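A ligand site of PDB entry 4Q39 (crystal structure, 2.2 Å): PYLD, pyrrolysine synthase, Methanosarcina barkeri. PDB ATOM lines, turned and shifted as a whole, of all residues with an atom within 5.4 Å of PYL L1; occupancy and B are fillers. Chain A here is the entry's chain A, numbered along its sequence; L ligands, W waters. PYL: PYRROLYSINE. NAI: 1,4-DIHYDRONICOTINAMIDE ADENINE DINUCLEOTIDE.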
ATOM      1  N   ALA A   3     -10.863 -15.808  14.683  1.00  0.00           N
ATOM      2  CA  ALA A   3     -12.202 -16.300  14.357  1.00  0.00           C
ATOM      3  C   ALA A   3     -12.367 -17.661  15.008  1.00  0.00           C
ATOM      4  O   ALA A   3     -11.976 -18.686  14.420  1.00  0.00           O
ATOM      5  CB  ALA A   3     -12.375 -16.405  12.846  1.00  0.00           C
ATOM      6  N   LEU A   4     -12.886 -17.678  16.228  1.00  0.00           N
ATOM      7  CA  LEU A   4     -12.984 -18.918  16.990  1.00  0.00           C
ATOM      8  C   LEU A   4     -14.341 -19.618  16.804  1.00  0.00           C
ATOM      9  O   LEU A   4     -15.380 -18.978  16.731  1.00  0.00           O
ATOM     10  CB  LEU A   4     -12.768 -18.653  18.467  1.00  0.00           C
ATOM     11  CG  LEU A   4     -11.416 -18.037  18.860  1.00  0.00           C
ATOM     12  CD1 LEU A   4     -11.218 -18.155  20.362  1.00  0.00           C
ATOM     13  CD2 LEU A   4     -10.239 -18.648  18.115  1.00  0.00           C
ATOM     14  N   LEU A   5     -14.300 -20.940  16.770  1.00  0.00           N
ATOM     15  CA  LEU A   5     -15.516 -21.735  16.757  1.00  0.00           C
ATOM     16  C   LEU A   5     -16.458 -21.314  17.861  1.00  0.00           C
ATOM     17  O   LEU A   5     -16.009 -20.817  18.898  1.00  0.00           O
ATOM     18  CB  LEU A   5     -15.172 -23.213  16.953  1.00  0.00           C
ATOM     19  CG  LEU A   5     -14.477 -23.902  15.786  1.00  0.00           C
ATOM     20  CD1 LEU A   5     -14.040 -25.275  16.215  1.00  0.00           C
ATOM     21  CD2 LEU A   5     -15.447 -23.984  14.613  1.00  0.00           C
ATOM     22  N   VAL A  52      -7.670 -32.806  25.905  1.00  0.00           N
ATOM     23  CA  VAL A  52      -7.541 -31.997  27.113  1.00  0.00           C
ATOM     24  C   VAL A  52      -8.221 -30.649  26.967  1.00  0.00           C
ATOM     25  O   VAL A  52      -7.774 -29.796  26.184  1.00  0.00           O
ATOM     26  CB  VAL A  52      -6.054 -31.746  27.500  1.00  0.00           C
ATOM     27  CG1 VAL A  52      -5.969 -30.947  28.786  1.00  0.00           C
ATOM     28  CG2 VAL A  52      -5.294 -33.048  27.606  1.00  0.00           C
ATOM     29  N   PRO A  53      -9.299 -30.422  27.724  1.00  0.00           N
ATOM     30  CA  PRO A  53      -9.900 -29.104  27.703  1.00  0.00           C
ATOM     31  C   PRO A  53      -8.915 -28.032  28.207  1.00  0.00           C
ATOM     32  O   PRO A  53      -8.110 -28.297  29.108  1.00  0.00           O
ATOM     33  CB  PRO A  53     -11.088 -29.236  28.652  1.00  0.00           C
ATOM     34  CG  PRO A  53     -11.356 -30.706  28.732  1.00  0.00           C
ATOM     35  CD  PRO A  53      -9.985 -31.307  28.684  1.00  0.00           C
ATOM     36  N   VAL A  54      -9.001 -26.839  27.625  1.00  0.00           N
ATOM     37  CA  VAL A  54      -8.093 -25.745  27.931  1.00  0.00           C
ATOM     38  C   VAL A  54      -8.901 -24.477  28.222  1.00  0.00           C
ATOM     39  O   VAL A  54      -9.743 -24.100  27.430  1.00  0.00           O
ATOM     40  CB  VAL A  54      -7.120 -25.572  26.744  1.00  0.00           C
ATOM     41  CG1 VAL A  54      -6.363 -24.237  26.815  1.00  0.00           C
ATOM     42  CG2 VAL A  54      -6.127 -26.730  26.742  1.00  0.00           C
ATOM     43  N   THR A  55      -8.662 -23.881  29.385  1.00  0.00           N
ATOM     44  CA  THR A  55      -9.342 -22.665  29.880  1.00  0.00           C
ATOM     45  C   THR A  55      -8.634 -21.363  29.545  1.00  0.00           C
ATOM     46  O   THR A  55      -9.108 -20.268  29.868  1.00  0.00           O
ATOM     47  CB  THR A  55      -9.511 -22.697  31.412  1.00  0.00           C
ATOM     48  OG1 THR A  55      -8.235 -22.611  32.039  1.00  0.00           O
ATOM     49  CG2 THR A  55     -10.194 -23.980  31.877  1.00  0.00           C
ATOM     50  N   SER A  56      -7.519 -21.460  28.852  1.00  0.00           N
ATOM     51  CA  SER A  56      -6.768 -20.298  28.428  1.00  0.00           C
ATOM     52  C   SER A  56      -7.598 -19.345  27.564  1.00  0.00           C
ATOM     53  O   SER A  56      -8.452 -19.792  26.784  1.00  0.00           O
ATOM     54  CB  SER A  56      -5.527 -20.786  27.646  1.00  0.00           C
ATOM     55  OG  SER A  56      -5.084 -19.808  26.733  1.00  0.00           O
ATOM     56  N   GLY A  59     -11.333 -19.274  26.699  1.00  0.00           N
ATOM     57  CA  GLY A  59     -11.759 -20.370  27.553  1.00  0.00           C
ATOM     58  C   GLY A  59     -12.303 -21.559  26.765  1.00  0.00           C
ATOM     59  O   GLY A  59     -12.197 -21.615  25.541  1.00  0.00           O
ATOM     60  N   ILE A  60     -12.869 -22.486  27.520  1.00  0.00           N
ATOM     61  CA  ILE A  60     -13.469 -23.682  27.014  1.00  0.00           C
ATOM     62  C   ILE A  60     -14.637 -23.324  26.103  1.00  0.00           C
ATOM     63  O   ILE A  60     -15.503 -22.553  26.477  1.00  0.00           O
ATOM     64  CB  ILE A  60     -13.950 -24.582  28.155  1.00  0.00           C
ATOM     65  CG1 ILE A  60     -12.726 -25.208  28.833  1.00  0.00           C
ATOM     66  CG2 ILE A  60     -14.853 -25.688  27.592  1.00  0.00           C
ATOM     67  CD1 ILE A  60     -13.026 -26.208  29.934  1.00  0.00           C
ATOM     68  N   ILE A  61     -14.633 -23.889  24.912  1.00  0.00           N
ATOM     69  CA  ILE A  61     -15.731 -23.695  23.986  1.00  0.00           C
ATOM     70  C   ILE A  61     -16.699 -24.865  24.099  1.00  0.00           C
ATOM     71  O   ILE A  61     -16.331 -26.035  23.876  1.00  0.00           O
ATOM     72  CB  ILE A  61     -15.208 -23.511  22.545  1.00  0.00           C
ATOM     73  CG1 ILE A  61     -14.300 -22.280  22.464  1.00  0.00           C
ATOM     74  CG2 ILE A  61     -16.344 -23.422  21.556  1.00  0.00           C
ATOM     75  CD1 ILE A  61     -13.670 -22.062  21.096  1.00  0.00           C
ATOM     76  N   PHE A  64     -16.677 -28.355  22.118  1.00  0.00           N
ATOM     77  CA  PHE A  64     -15.396 -28.550  21.418  1.00  0.00           C
ATOM     78  C   PHE A  64     -14.804 -29.918  21.720  1.00  0.00           C
ATOM     79  O   PHE A  64     -14.553 -30.709  20.802  1.00  0.00           O
ATOM     80  CB  PHE A  64     -14.413 -27.463  21.780  1.00  0.00           C
ATOM     81  CG  PHE A  64     -13.128 -27.532  21.031  1.00  0.00           C
ATOM     82  CD1 PHE A  64     -13.042 -27.082  19.726  1.00  0.00           C
ATOM     83  CD2 PHE A  64     -11.978 -28.008  21.647  1.00  0.00           C
ATOM     84  CE1 PHE A  64     -11.854 -27.150  19.027  1.00  0.00           C
ATOM     85  CE2 PHE A  64     -10.768 -28.047  20.946  1.00  0.00           C
ATOM     86  CZ  PHE A  64     -10.703 -27.622  19.635  1.00  0.00           C
ATOM     87  N   SER A  65     -14.585 -30.180  23.000  1.00  0.00           N
ATOM     88  CA  SER A  65     -14.025 -31.452  23.392  1.00  0.00           C
ATOM     89  C   SER A  65     -14.955 -32.618  23.033  1.00  0.00           C
ATOM     90  O   SER A  65     -14.479 -33.653  22.559  1.00  0.00           O
ATOM     91  CB  SER A  65     -13.640 -31.471  24.880  1.00  0.00           C
ATOM     92  OG  SER A  65     -14.798 -31.445  25.745  1.00  0.00           O
ATOM     93  N   ALA A 104      -6.108 -27.484  22.439  1.00  0.00           N
ATOM     94  CA  ALA A 104      -6.160 -26.175  21.787  1.00  0.00           C
ATOM     95  C   ALA A 104      -6.280 -24.999  22.749  1.00  0.00           C
ATOM     96  O   ALA A 104      -7.114 -25.012  23.646  1.00  0.00           O
ATOM     97  CB  ALA A 104      -7.336 -26.129  20.802  1.00  0.00           C
ATOM     98  N   ASP A 105      -5.476 -23.954  22.527  1.00  0.00           N
ATOM     99  CA  ASP A 105      -5.780 -22.620  23.077  1.00  0.00           C
ATOM    100  C   ASP A 105      -6.307 -21.753  21.928  1.00  0.00           C
ATOM    101  O   ASP A 105      -6.633 -22.291  20.859  1.00  0.00           O
ATOM    102  CB  ASP A 105      -4.614 -22.029  23.891  1.00  0.00           C
ATOM    103  CG  ASP A 105      -3.375 -21.660  23.089  1.00  0.00           C
ATOM    104  OD1 ASP A 105      -3.389 -21.500  21.852  1.00  0.00           O
ATOM    105  OD2 ASP A 105      -2.313 -21.513  23.764  1.00  0.00           O
ATOM    106  N   ASP A 106      -6.426 -20.439  22.138  1.00  0.00           N
ATOM    107  CA  ASP A 106      -7.071 -19.589  21.152  1.00  0.00           C
ATOM    108  C   ASP A 106      -6.236 -19.399  19.901  1.00  0.00           C
ATOM    109  O   ASP A 106      -6.777 -19.021  18.859  1.00  0.00           O
ATOM    110  CB  ASP A 106      -7.451 -18.229  21.758  1.00  0.00           C
ATOM    111  CG  ASP A 106      -8.522 -18.360  22.822  1.00  0.00           C
ATOM    112  OD1 ASP A 106      -9.133 -19.450  22.920  1.00  0.00           O
ATOM    113  OD2 ASP A 106      -8.742 -17.399  23.559  1.00  0.00           O
ATOM    114  N   PHE A 109      -4.111 -25.133  17.874  1.00  0.00           N
ATOM    115  CA  PHE A 109      -4.723 -26.422  18.120  1.00  0.00           C
ATOM    116  C   PHE A 109      -3.724 -27.443  17.640  1.00  0.00           C
ATOM    117  O   PHE A 109      -3.318 -27.394  16.496  1.00  0.00           O
ATOM    118  CB  PHE A 109      -6.096 -26.513  17.391  1.00  0.00           C
ATOM    119  CG  PHE A 109      -6.735 -27.882  17.395  1.00  0.00           C
ATOM    120  CD1 PHE A 109      -6.511 -28.799  18.412  1.00  0.00           C
ATOM    121  CD2 PHE A 109      -7.599 -28.257  16.375  1.00  0.00           C
ATOM    122  CE1 PHE A 109      -7.105 -30.048  18.419  1.00  0.00           C
ATOM    123  CE2 PHE A 109      -8.199 -29.506  16.370  1.00  0.00           C
ATOM    124  CZ  PHE A 109      -7.971 -30.398  17.401  1.00  0.00           C
ATOM    125  N   ASN A 122      -3.078 -27.379  13.638  1.00  0.00           N
ATOM    126  CA  ASN A 122      -4.344 -27.397  12.888  1.00  0.00           C
ATOM    127  C   ASN A 122      -4.324 -26.567  11.609  1.00  0.00           C
ATOM    128  O   ASN A 122      -4.920 -26.945  10.594  1.00  0.00           O
ATOM    129  CB  ASN A 122      -5.458 -26.900  13.780  1.00  0.00           C
ATOM    130  CG  ASN A 122      -6.783 -26.826  13.079  1.00  0.00           C
ATOM    131  OD1 ASN A 122      -7.274 -25.737  12.822  1.00  0.00           O
ATOM    132  ND2 ASN A 122      -7.379 -27.980  12.803  1.00  0.00           N
ATOM    133  N   PRO A 247     -16.780 -28.051  10.104  1.00  0.00           N
ATOM    134  CA  PRO A 247     -16.150 -27.069  11.019  1.00  0.00           C
ATOM    135  C   PRO A 247     -14.923 -27.509  11.818  1.00  0.00           C
ATOM    136  O   PRO A 247     -14.223 -26.658  12.368  1.00  0.00           O
ATOM    137  CB  PRO A 247     -17.286 -26.703  11.975  1.00  0.00           C
ATOM    138  CG  PRO A 247     -18.117 -27.961  12.000  1.00  0.00           C
ATOM    139  CD  PRO A 247     -18.113 -28.438  10.581  1.00  0.00           C
ATOM    140  N   LEU A 248     -14.634 -28.807  11.880  1.00  0.00           N
ATOM    141  CA  LEU A 248     -13.544 -29.282  12.749  1.00  0.00           C
ATOM    142  C   LEU A 248     -12.902 -30.627  12.350  1.00  0.00           C
ATOM    143  O   LEU A 248     -11.682 -30.776  12.453  1.00  0.00           O
ATOM    144  CB  LEU A 248     -14.047 -29.326  14.198  1.00  0.00           C
ATOM    145  CG  LEU A 248     -13.046 -29.660  15.307  1.00  0.00           C
ATOM    146  CD1 LEU A 248     -11.920 -28.634  15.356  1.00  0.00           C
ATOM    147  CD2 LEU A 248     -13.751 -29.717  16.653  1.00  0.00           C
HETATM  148  CB2 PYL L   1      -9.591 -25.283  15.968  1.00  0.00           C
HETATM  149  CG2 PYL L   1     -10.673 -24.304  15.606  1.00  0.00           C
HETATM  150  CD2 PYL L   1     -11.058 -24.344  14.134  1.00  0.00           C
HETATM  151  CE2 PYL L   1     -11.233 -22.888  13.811  1.00  0.00           C
HETATM  152  N2  PYL L   1     -10.828 -22.127  14.749  1.00  0.00           N
HETATM  153  CA2 PYL L   1     -10.195 -22.880  15.830  1.00  0.00           C
HETATM  154  C2  PYL L   1     -10.623 -22.502  17.194  1.00  0.00           C
HETATM  155  O2  PYL L   1     -11.789 -22.165  17.339  1.00  0.00           O
HETATM  156  NZ  PYL L   1      -9.700 -22.605  18.158  1.00  0.00           N
HETATM  157  CE  PYL L   1     -10.009 -22.297  19.555  1.00  0.00           C
HETATM  158  CD  PYL L   1     -10.374 -23.550  20.327  1.00  0.00           C
HETATM  159  CG  PYL L   1     -10.273 -23.362  21.821  1.00  0.00           C
HETATM  160  CB  PYL L   1     -10.640 -24.630  22.562  1.00  0.00           C
HETATM  161  CA  PYL L   1     -10.849 -24.421  24.064  1.00  0.00           C
HETATM  162  C   PYL L   1     -11.303 -25.716  24.682  1.00  0.00           C
HETATM  163  OXT PYL L   1     -12.537 -25.980  24.657  1.00  0.00           O
HETATM  164  O   PYL L   1     -10.448 -26.520  25.171  1.00  0.00           O
HETATM  165  N   PYL L   1      -9.616 -23.960  24.674  1.00  0.00           N
HETATM  166  PA  NAI L   2      -6.539 -15.865   8.847  1.00  0.00           P
HETATM  167  O1A NAI L   2      -7.154 -14.633   9.420  1.00  0.00           O
HETATM  168  O2A NAI L   2      -5.116 -16.230   9.047  1.00  0.00           O
HETATM  169  O5B NAI L   2      -6.738 -15.804   7.258  1.00  0.00           O
HETATM  170  C5B NAI L   2      -7.976 -15.368   6.718  1.00  0.00           C
HETATM  171  C4B NAI L   2      -7.628 -14.560   5.468  1.00  0.00           C
HETATM  172  O4B NAI L   2      -8.801 -14.296   4.724  1.00  0.00           O
HETATM  173  C3B NAI L   2      -7.022 -13.201   5.831  1.00  0.00           C
HETATM  174  O3B NAI L   2      -5.763 -13.089   5.195  1.00  0.00           O
HETATM  175  C2B NAI L   2      -7.975 -12.159   5.310  1.00  0.00           C
HETATM  176  O2B NAI L   2      -7.276 -11.077   4.697  1.00  0.00           O
HETATM  177  C1B NAI L   2      -8.679 -12.954   4.238  1.00  0.00           C
HETATM  178  N9A NAI L   2      -9.998 -12.424   3.870  1.00  0.00           N
HETATM  179  C8A NAI L   2     -11.024 -12.041   4.651  1.00  0.00           C
HETATM  180  N7A NAI L   2     -12.082 -11.647   3.883  1.00  0.00           N
HETATM  181  C5A NAI L   2     -11.716 -11.782   2.611  1.00  0.00           C
HETATM  182  C6A NAI L   2     -12.310 -11.540   1.291  1.00  0.00           C
HETATM  183  N6A NAI L   2     -13.550 -11.071   1.159  1.00  0.00           N
HETATM  184  N1A NAI L   2     -11.580 -11.838   0.211  1.00  0.00           N
HETATM  185  C2A NAI L   2     -10.342 -12.325   0.288  1.00  0.00           C
HETATM  186  N3A NAI L   2      -9.731 -12.542   1.440  1.00  0.00           N
HETATM  187  C4A NAI L   2     -10.362 -12.296   2.604  1.00  0.00           C
HETATM  188  O3  NAI L   2      -7.604 -17.022   9.280  1.00  0.00           O
HETATM  189  PN  NAI L   2      -7.224 -18.575   9.203  1.00  0.00           P
HETATM  190  O1N NAI L   2      -6.495 -19.092  10.415  1.00  0.00           O
HETATM  191  O2N NAI L   2      -6.569 -18.860   7.851  1.00  0.00           O
HETATM  192  O5D NAI L   2      -8.720 -19.187   9.265  1.00  0.00           O
HETATM  193  C5D NAI L   2      -9.574 -18.993   8.157  1.00  0.00           C
HETATM  194  C4D NAI L   2     -10.947 -19.539   8.508  1.00  0.00           C
HETATM  195  O4D NAI L   2     -10.960 -20.960   8.698  1.00  0.00           O
HETATM  196  C3D NAI L   2     -11.505 -18.976   9.784  1.00  0.00           C
HETATM  197  O3D NAI L   2     -12.916 -18.863   9.557  1.00  0.00           O
HETATM  198  C2D NAI L   2     -11.293 -20.050  10.820  1.00  0.00           C
HETATM  199  O2D NAI L   2     -12.305 -19.995  11.809  1.00  0.00           O
HETATM  200  C1D NAI L   2     -11.524 -21.282   9.989  1.00  0.00           C
HETATM  201  N1N NAI L   2     -10.918 -22.551  10.358  1.00  0.00           N
HETATM  202  C2N NAI L   2     -11.658 -23.635  10.102  1.00  0.00           C
HETATM  203  C3N NAI L   2     -11.185 -24.915  10.324  1.00  0.00           C
HETATM  204  C7N NAI L   2     -12.042 -26.103   9.990  1.00  0.00           C
HETATM  205  O7N NAI L   2     -11.647 -27.230  10.335  1.00  0.00           O
HETATM  206  N7N NAI L   2     -13.169 -25.966   9.291  1.00  0.00           N
HETATM  207  C4N NAI L   2      -9.796 -25.126  10.862  1.00  0.00           C
HETATM  208  C5N NAI L   2      -9.076 -23.873  11.077  1.00  0.00           C
HETATM  209  C6N NAI L   2      -9.653 -22.637  10.812  1.00  0.00           C
HETATM  210  O   HOH W   1      -8.615 -21.562  24.674  1.00  0.00           O
HETATM  211  O   HOH W   2      -6.971 -23.344  18.268  1.00  0.00           O
HETATM  212  O   HOH W   3      -8.360 -28.277  24.173  1.00  0.00           O
HETATM  213  O   HOH W   4     -13.139 -28.386  25.843  1.00  0.00           O
HETATM  214  O   HOH W   5      -8.860 -19.865  14.385  1.00  0.00           O
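The backbone NH (N) of Val 54 is in hydrogen-bond range of an oxygen (O) of PYL L1, 2.9 Å away.
The backbone carbonyl oxygen (O) of Val 54 lies within hydrogen-bond range of a nitrogen (N) of PYL L1, at 2.8 Å.
The backbone NH (N) of Leu 5 is in hydrogen-bond range of an oxygen (O2) of PYL L1.
A nitrogen (N) of PYL L1 sits at hydrogen-bond distance from the backbone carbonyl oxygen (O) of Ala 104 (2.9 Å).
OXT of PYL L1 lies within hydrogen-bond range of N of Ile 61 (3.0 Å).
O of Ala 3 sits at hydrogen-bond distance from O2D of NAI L2, 2.9 Å away.
The backbone carbonyl oxygen (O) of Pro 247 lies close to a nitrogen (N7N) of NAI L2 (3.3 Å).
N of Asn 122 sits at hydrogen-bond distance from O of Phe 109.
Ala 3 touches PYL L1 (O to N2, 3.6 Å).
Leu 4 touches PYL L1 (CA to O2, 3.5 Å).
Pro 53 touches PYL L1.
Gly 59 touches PYL L1 (O to CA, 3.4 Å).
Ile 60 touches PYL L1.
CD2 of Phe 64 touches OXT of PYL L1, at 3.7 Å.
Asp 105 touches PYL L1 (O to CE, 3.6 Å).
Phe 109 touches PYL L1.
Asn 122 touches PYL L1.
Hydrophobic or aromatic side chains that line PYL L1: Leu 4, Leu 5, Val 54, Ile 60, Ile 61, Phe 64 and Phe 109.
13 residues have an atom within 4 Å of PYL L1: Ala 3, Leu 4, Leu 5, Pro 53, Val 54, Gly 59, Ile 60, Ile 61, Phe 64, Ala 104, Asp 105, Phe 109 and Asn 122.
Water W1 lies within hydrogen-bond range of N of PYL L1 (2.6 Å), O of Ser 56 (2.8 Å) and OD1 of Asp 106 (2.8 Å).
Water W4 lies within hydrogen-bond range of OXT of PYL L1 (2.7 Å) and OG of Ser 65 (3.5 Å).
Water W2 lies within hydrogen-bond range of O of Asp 105, NZ of PYL L1 and N of Phe 109.
Water W3 lies within hydrogen-bond range of O of Val 52 (2.6 Å), O of PYL L1 (2.9 Å) and N of Ala 104 (3.0 Å).
Water W5 bridges a nitrogen (N2) of PYL L1 (3.0 Å) and the backbone carbonyl oxygen of Ala 3 (3.3 Å).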
